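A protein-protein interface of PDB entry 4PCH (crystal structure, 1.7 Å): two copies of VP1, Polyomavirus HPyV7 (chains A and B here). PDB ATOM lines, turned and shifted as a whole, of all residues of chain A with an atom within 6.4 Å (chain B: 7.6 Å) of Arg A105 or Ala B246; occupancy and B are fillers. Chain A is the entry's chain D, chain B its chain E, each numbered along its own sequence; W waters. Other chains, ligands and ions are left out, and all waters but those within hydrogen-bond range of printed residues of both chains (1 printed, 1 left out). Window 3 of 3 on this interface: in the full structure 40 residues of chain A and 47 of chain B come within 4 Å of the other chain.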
ATOM      1  N   TYR A 103     -15.529  20.248  18.275  1.00  0.00           N
ATOM      2  CA  TYR A 103     -14.878  19.352  17.348  1.00  0.00           C
ATOM      3  C   TYR A 103     -15.814  18.881  16.259  1.00  0.00           C
ATOM      4  O   TYR A 103     -17.019  18.764  16.418  1.00  0.00           O
ATOM      5  CB  TYR A 103     -14.181  18.195  18.043  1.00  0.00           C
ATOM      6  CG  TYR A 103     -15.086  17.253  18.793  1.00  0.00           C
ATOM      7  CD1 TYR A 103     -15.360  17.451  20.146  1.00  0.00           C
ATOM      8  CD2 TYR A 103     -15.646  16.149  18.161  1.00  0.00           C
ATOM      9  CE1 TYR A 103     -16.170  16.574  20.841  1.00  0.00           C
ATOM     10  CE2 TYR A 103     -16.459  15.262  18.854  1.00  0.00           C
ATOM     11  CZ  TYR A 103     -16.721  15.484  20.188  1.00  0.00           C
ATOM     12  OH  TYR A 103     -17.532  14.612  20.878  1.00  0.00           O
ATOM     13  N   GLN A 104     -15.219  18.708  15.084  1.00  0.00           N
ATOM     14  CA  GLN A 104     -15.965  18.281  13.903  1.00  0.00           C
ATOM     15  C   GLN A 104     -15.611  16.832  13.611  1.00  0.00           C
ATOM     16  O   GLN A 104     -14.496  16.560  13.147  1.00  0.00           O
ATOM     17  CB  GLN A 104     -15.628  19.139  12.686  1.00  0.00           C
ATOM     18  CG  GLN A 104     -16.384  18.678  11.447  1.00  0.00           C
ATOM     19  CD  GLN A 104     -15.996  19.467  10.215  1.00  0.00           C
ATOM     20  OE1 GLN A 104     -14.872  19.964  10.102  1.00  0.00           O
ATOM     21  NE2 GLN A 104     -16.922  19.602   9.301  1.00  0.00           N
ATOM     22  N   ARG A 105     -16.543  15.917  13.873  1.00  0.00           N
ATOM     23  CA  ARG A 105     -16.295  14.480  13.690  1.00  0.00           C
ATOM     24  C   ARG A 105     -15.908  14.151  12.246  1.00  0.00           C
ATOM     25  O   ARG A 105     -15.015  13.351  12.024  1.00  0.00           O
ATOM     26  CB  ARG A 105     -17.508  13.624  14.082  1.00  0.00           C
ATOM     27  CG  ARG A 105     -17.702  13.439  15.558  1.00  0.00           C
ATOM     28  CD  ARG A 105     -18.678  12.307  15.859  1.00  0.00           C
ATOM     29  NE  ARG A 105     -18.919  12.232  17.295  1.00  0.00           N
ATOM     30  CZ  ARG A 105     -19.982  12.719  17.940  1.00  0.00           C
ATOM     31  NH1 ARG A 105     -20.050  12.577  19.258  1.00  0.00           N
ATOM     32  NH2 ARG A 105     -20.986  13.324  17.301  1.00  0.00           N
ATOM     33  N   ALA A 106     -16.551  14.805  11.277  1.00  0.00           N
ATOM     34  CA  ALA A 106     -16.364  14.435   9.860  1.00  0.00           C
ATOM     35  C   ALA A 106     -14.924  14.631   9.391  1.00  0.00           C
ATOM     36  O   ALA A 106     -14.477  13.966   8.455  1.00  0.00           O
ATOM     37  CB  ALA A 106     -17.323  15.209   8.959  1.00  0.00           C
ATOM     38  N   ASN A 107     -14.209  15.565  10.019  1.00  0.00           N
ATOM     39  CA  ASN A 107     -12.801  15.796   9.710  1.00  0.00           C
ATOM     40  C   ASN A 107     -11.865  15.399  10.829  1.00  0.00           C
ATOM     41  O   ASN A 107     -10.682  15.709  10.756  1.00  0.00           O
ATOM     42  CB  ASN A 107     -12.579  17.264   9.336  1.00  0.00           C
ATOM     43  CG  ASN A 107     -12.992  17.572   7.907  1.00  0.00           C
ATOM     44  OD1 ASN A 107     -12.698  16.805   6.975  1.00  0.00           O
ATOM     45  ND2 ASN A 107     -13.660  18.690   7.720  1.00  0.00           N
ATOM     46  N   GLY A 108     -12.377  14.694  11.845  1.00  0.00           N
ATOM     47  CA  GLY A 108     -11.582  14.200  12.959  1.00  0.00           C
ATOM     48  C   GLY A 108     -10.687  15.218  13.615  1.00  0.00           C
ATOM     49  O   GLY A 108      -9.540  14.918  13.949  1.00  0.00           O
ATOM     50  N   THR A 109     -11.184  16.435  13.784  1.00  0.00           N
ATOM     51  CA  THR A 109     -10.339  17.515  14.294  1.00  0.00           C
ATOM     52  C   THR A 109     -11.168  18.658  14.881  1.00  0.00           C
ATOM     53  O   THR A 109     -12.395  18.642  14.863  1.00  0.00           O
ATOM     54  CB  THR A 109      -9.334  17.999  13.224  1.00  0.00           C
ATOM     55  OG1 THR A 109      -8.249  18.684  13.859  1.00  0.00           O
ATOM     56  CG2 THR A 109      -9.999  18.885  12.179  1.00  0.00           C
ATOM     57  N   PRO A 242     -19.318  18.198  20.117  1.00  0.00           N
ATOM     58  CA  PRO A 242     -19.405  18.187  18.644  1.00  0.00           C
ATOM     59  C   PRO A 242     -20.144  19.366  18.056  1.00  0.00           C
ATOM     60  O   PRO A 242     -21.092  19.883  18.648  1.00  0.00           O
ATOM     61  CB  PRO A 242     -20.136  16.879  18.330  1.00  0.00           C
ATOM     62  CG  PRO A 242     -20.885  16.565  19.597  1.00  0.00           C
ATOM     63  CD  PRO A 242     -20.075  17.091  20.725  1.00  0.00           C
ATOM     64  N   THR A 243     -19.703  19.780  16.872  1.00  0.00           N
ATOM     65  CA  THR A 243     -20.350  20.857  16.136  1.00  0.00           C
ATOM     66  C   THR A 243     -20.192  20.599  14.637  1.00  0.00           C
ATOM     67  O   THR A 243     -19.643  19.578  14.233  1.00  0.00           O
ATOM     68  CB  THR A 243     -19.842  22.231  16.562  1.00  0.00           C
ATOM     69  OG1 THR A 243     -20.662  23.262  15.983  1.00  0.00           O
ATOM     70  CG2 THR A 243     -18.377  22.428  16.150  1.00  0.00           C
ATOM     71  N   SER A 245     -22.486  19.720  12.666  1.00  0.00           N
ATOM     72  CA  SER A 245     -23.328  18.584  12.318  1.00  0.00           C
ATOM     73  C   SER A 245     -24.765  18.912  12.727  1.00  0.00           C
ATOM     74  O   SER A 245     -24.981  19.677  13.659  1.00  0.00           O
ATOM     75  CB  SER A 245     -22.842  17.312  13.023  1.00  0.00           C
ATOM     76  OG  SER A 245     -23.491  16.174  12.488  1.00  0.00           O
ATOM     77  N   TYR A 248     -26.413  19.399  16.356  1.00  0.00           N
ATOM     78  CA  TYR A 248     -25.835  20.420  17.228  1.00  0.00           C
ATOM     79  C   TYR A 248     -25.986  21.825  16.679  1.00  0.00           C
ATOM     80  O   TYR A 248     -25.374  22.773  17.193  1.00  0.00           O
ATOM     81  CB  TYR A 248     -24.358  20.097  17.507  1.00  0.00           C
ATOM     82  CG  TYR A 248     -24.180  18.622  17.763  1.00  0.00           C
ATOM     83  CD1 TYR A 248     -24.744  18.015  18.878  1.00  0.00           C
ATOM     84  CD2 TYR A 248     -23.518  17.826  16.855  1.00  0.00           C
ATOM     85  CE1 TYR A 248     -24.629  16.635  19.085  1.00  0.00           C
ATOM     86  CE2 TYR A 248     -23.393  16.459  17.046  1.00  0.00           C
ATOM     87  CZ  TYR A 248     -23.948  15.869  18.157  1.00  0.00           C
ATOM     88  OH  TYR A 248     -23.806  14.515  18.309  1.00  0.00           O
ATOM     89  N   MET B  49      -9.857  16.374  21.896  1.00  0.00           N
ATOM     90  CA  MET B  49     -11.069  17.036  21.499  1.00  0.00           C
ATOM     91  C   MET B  49     -11.860  17.500  22.724  1.00  0.00           C
ATOM     92  O   MET B  49     -13.073  17.669  22.633  1.00  0.00           O
ATOM     93  CB  MET B  49     -11.923  16.087  20.651  1.00  0.00           C
ATOM     94  CG  MET B  49     -11.261  15.632  19.356  1.00  0.00           C
ATOM     95  SD  MET B  49     -10.841  16.915  18.136  1.00  0.00           S
ATOM     96  CE  MET B  49      -9.092  17.094  18.432  1.00  0.00           C
ATOM     97  N   ARG B 105      -7.587   9.041   4.754  1.00  0.00           N
ATOM     98  CA  ARG B 105      -8.108   7.868   4.067  1.00  0.00           C
ATOM     99  C   ARG B 105      -9.119   8.230   3.004  1.00  0.00           C
ATOM    100  O   ARG B 105      -9.049   7.729   1.869  1.00  0.00           O
ATOM    101  CB  ARG B 105      -8.761   6.889   5.059  1.00  0.00           C
ATOM    102  CG  ARG B 105      -7.906   5.684   5.403  1.00  0.00           C
ATOM    103  CD  ARG B 105      -8.742   4.603   6.085  1.00  0.00           C
ATOM    104  NE  ARG B 105      -9.573   5.219   7.109  1.00  0.00           N
ATOM    105  CZ  ARG B 105      -9.330   5.253   8.422  1.00  0.00           C
ATOM    106  NH1 ARG B 105     -10.170   5.905   9.193  1.00  0.00           N
ATOM    107  NH2 ARG B 105      -8.300   4.631   8.980  1.00  0.00           N
ATOM    108  N   THR B 243      -5.381  10.310   9.687  1.00  0.00           N
ATOM    109  CA  THR B 243      -5.788  11.512  10.353  1.00  0.00           C
ATOM    110  C   THR B 243      -6.909  12.177   9.575  1.00  0.00           C
ATOM    111  O   THR B 243      -7.256  11.742   8.474  1.00  0.00           O
ATOM    112  CB  THR B 243      -4.586  12.439  10.546  1.00  0.00           C
ATOM    113  OG1 THR B 243      -4.897  13.462  11.500  1.00  0.00           O
ATOM    114  CG2 THR B 243      -4.144  13.056   9.237  1.00  0.00           C
ATOM    115  N   LEU B 244      -7.443  13.253  10.147  1.00  0.00           N
ATOM    116  CA  LEU B 244      -8.642  13.930   9.624  1.00  0.00           C
ATOM    117  C   LEU B 244      -9.854  12.988   9.565  1.00  0.00           C
ATOM    118  O   LEU B 244     -10.760  13.148   8.752  1.00  0.00           O
ATOM    119  CB  LEU B 244      -8.368  14.630   8.279  1.00  0.00           C
ATOM    120  CG  LEU B 244      -7.315  15.738   8.375  1.00  0.00           C
ATOM    121  CD1 LEU B 244      -6.996  16.215   6.966  1.00  0.00           C
ATOM    122  CD2 LEU B 244      -7.755  16.928   9.224  1.00  0.00           C
ATOM    123  N   SER B 245      -9.878  11.999  10.457  1.00  0.00           N
ATOM    124  CA  SER B 245     -11.052  11.147  10.623  1.00  0.00           C
ATOM    125  C   SER B 245     -11.237  10.897  12.119  1.00  0.00           C
ATOM    126  O   SER B 245     -10.272  10.914  12.896  1.00  0.00           O
ATOM    127  CB  SER B 245     -10.912   9.823   9.847  1.00  0.00           C
ATOM    128  OG  SER B 245      -9.707   9.170  10.204  1.00  0.00           O
ATOM    129  N   ALA B 246     -12.487  10.713  12.525  1.00  0.00           N
ATOM    130  CA  ALA B 246     -12.849  10.712  13.950  1.00  0.00           C
ATOM    131  C   ALA B 246     -12.075   9.692  14.778  1.00  0.00           C
ATOM    132  O   ALA B 246     -11.684   9.964  15.943  1.00  0.00           O
ATOM    133  CB  ALA B 246     -14.334  10.477  14.104  1.00  0.00           C
ATOM    134  N   ASP B 247     -11.856   8.528  14.185  1.00  0.00           N
ATOM    135  CA  ASP B 247     -11.169   7.443  14.872  1.00  0.00           C
ATOM    136  C   ASP B 247      -9.782   7.845  15.406  1.00  0.00           C
ATOM    137  O   ASP B 247      -9.344   7.309  16.444  1.00  0.00           O
ATOM    138  CB  ASP B 247     -11.098   6.186  14.007  1.00  0.00           C
ATOM    139  CG  ASP B 247     -10.526   6.430  12.623  1.00  0.00           C
ATOM    140  OD1 ASP B 247     -10.291   7.593  12.237  1.00  0.00           O
ATOM    141  OD2 ASP B 247     -10.315   5.423  11.910  1.00  0.00           O
ATOM    142  N   TYR B 248      -9.109   8.772  14.707  1.00  0.00           N
ATOM    143  CA  TYR B 248      -7.776   9.217  15.075  1.00  0.00           C
ATOM    144  C   TYR B 248      -7.715  10.639  15.608  1.00  0.00           C
ATOM    145  O   TYR B 248      -6.622  11.231  15.742  1.00  0.00           O
ATOM    146  CB  TYR B 248      -6.862   9.040  13.871  1.00  0.00           C
ATOM    147  CG  TYR B 248      -6.394   7.625  13.776  1.00  0.00           C
ATOM    148  CD1 TYR B 248      -7.217   6.637  13.276  1.00  0.00           C
ATOM    149  CD2 TYR B 248      -5.134   7.258  14.247  1.00  0.00           C
ATOM    150  CE1 TYR B 248      -6.804   5.323  13.199  1.00  0.00           C
ATOM    151  CE2 TYR B 248      -4.711   5.942  14.180  1.00  0.00           C
ATOM    152  CZ  TYR B 248      -5.548   4.987  13.647  1.00  0.00           C
ATOM    153  OH  TYR B 248      -5.130   3.679  13.581  1.00  0.00           O
ATOM    154  N   SER B 249      -8.871  11.179  15.993  1.00  0.00           N
ATOM    155  CA  SER B 249      -8.919  12.561  16.490  1.00  0.00           C
ATOM    156  C   SER B 249      -8.122  12.758  17.775  1.00  0.00           C
ATOM    157  O   SER B 249      -7.641  13.857  18.033  1.00  0.00           O
ATOM    158  CB  SER B 249     -10.367  12.999  16.694  1.00  0.00           C
ATOM    159  OG  SER B 249     -11.030  12.184  17.628  1.00  0.00           O
ATOM    160  N   ASN B 250      -7.979  11.699  18.573  1.00  0.00           N
ATOM    161  CA  ASN B 250      -7.199  11.776  19.808  1.00  0.00           C
ATOM    162  C   ASN B 250      -5.681  11.840  19.582  1.00  0.00           C
ATOM    163  O   ASN B 250      -4.908  11.873  20.545  1.00  0.00           O
ATOM    164  CB  ASN B 250      -7.576  10.613  20.749  1.00  0.00           C
ATOM    165  N   GLN B 251      -5.246  11.825  18.326  1.00  0.00           N
ATOM    166  CA  GLN B 251      -3.832  11.993  17.987  1.00  0.00           C
ATOM    167  C   GLN B 251      -3.506  13.352  17.379  1.00  0.00           C
ATOM    168  O   GLN B 251      -2.324  13.659  17.195  1.00  0.00           O
ATOM    169  CB  GLN B 251      -3.377  10.901  17.015  1.00  0.00           C
ATOM    170  CG  GLN B 251      -3.378   9.523  17.639  1.00  0.00           C
ATOM    171  CD  GLN B 251      -2.655   8.479  16.804  1.00  0.00           C
ATOM    172  OE1 GLN B 251      -2.423   8.655  15.613  1.00  0.00           O
ATOM    173  NE2 GLN B 251      -2.291   7.380  17.443  1.00  0.00           N
HETATM  174  O   HOH W   1     -14.522  10.827  10.529  1.00  0.00           O
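Water W1 bridges N of Ala B246 (2.9 Å) and O of Arg A105 (3.0 Å).
Tyr A103 touches Met B49 (CD1 to O, 3.4 Å). Ala B246 touches Arg A105 (CB to O, 3.6 Å). O of Ala A106 touches O of Leu B244 (3.8 Å). O of Asn A107 touches N of Ser B245, at 3.8 Å. Gly A108 touches Leu B244. Ser B245 touches Gly A108. Gly A108 touches Ala B246 (CA to N, 3.6 Å). O of Gly A108 touches CB of Ser B249 (3.4 Å). SD of Met B49 touches C of Thr A109 (3.7 Å).
Printed residues of chain A that touch a printed residue of chain B: Tyr A103, Arg A105, Ala A106, Asn A107, Gly A108 and Thr A109. Hydrophobic or aromatic side chains of chain A that line the printed part of chain B: Tyr A103. Of the 11 printed residues of chain B, 5 touch a printed residue of chain A. Printed residues of chain B that touch a printed residue of chain A: Met B49, Leu B244, Ser B245, Ala B246 and Ser B249. Hydrophobic or aromatic side chains of chain B within 4 Å of the printed part of chain A: Met B49, Leu B244 and Ala B246. Among the printed residues, 10 pairs touch across the chains.
O of Asn A107 sits close to O of Leu B244 (3.3 Å).
O of Tyr A103 lies within hydrogen-bond range of N of Thr A243, 2.9 Å away. The side-chain amide oxygen (OE1) of Gln A104 lies within hydrogen-bond range of the side-chain amide nitrogen (ND2) of Asn A107. The backbone carbonyl oxygen (O) of Thr A109 is in hydrogen-bond range of the backbone NH (N) of Gln A104 (2.8 Å). NH2 of Arg A105 lies within hydrogen-bond range of OH of Tyr A248 (3.2 Å). NH1 of Arg B105 lies within hydrogen-bond range of OG of Ser B245 (3.4 Å). OG of Ser B245 is in hydrogen-bond range of OD1 of Asp B247.
Positions printed for both chains: 105, 243, 245 and 248. Of the 10 pairs that touch across the chains among the printed residues, none has its exchanged pair printed and touching as well.
Arg A105 touches one residue of chain B. Printed residues of chain A within 4 Å of Ala B246: Arg A105 (3.6 Å) and Gly A108 (3.6 Å). Printed residues of chain A within 4 Å of Ser B245: Asn A107 and Gly A108. Printed residues of chain B within 4 Å of Asn A107: Leu B244 and Ser B245. Printed residues of chain A within 4 Å of Ser B249: Gly A108 (3.4 Å). Of the printed residues of chain A, Met B49 touches Tyr A103 and Thr A109. Printed residues of chain B within 4 Å of Gly A108: Leu B244 (3.8 Å), Ser B245 (3.4 Å), Ala B246 (3.6 Å) and Ser B249 (3.4 Å). The nearest printed residue of chain A that does not touch Ala B246 is Asn A107 (5.0 Å). The nearest printed residue of chain B that does not touch Asn A107 is Ala B246 (5.0 Å).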
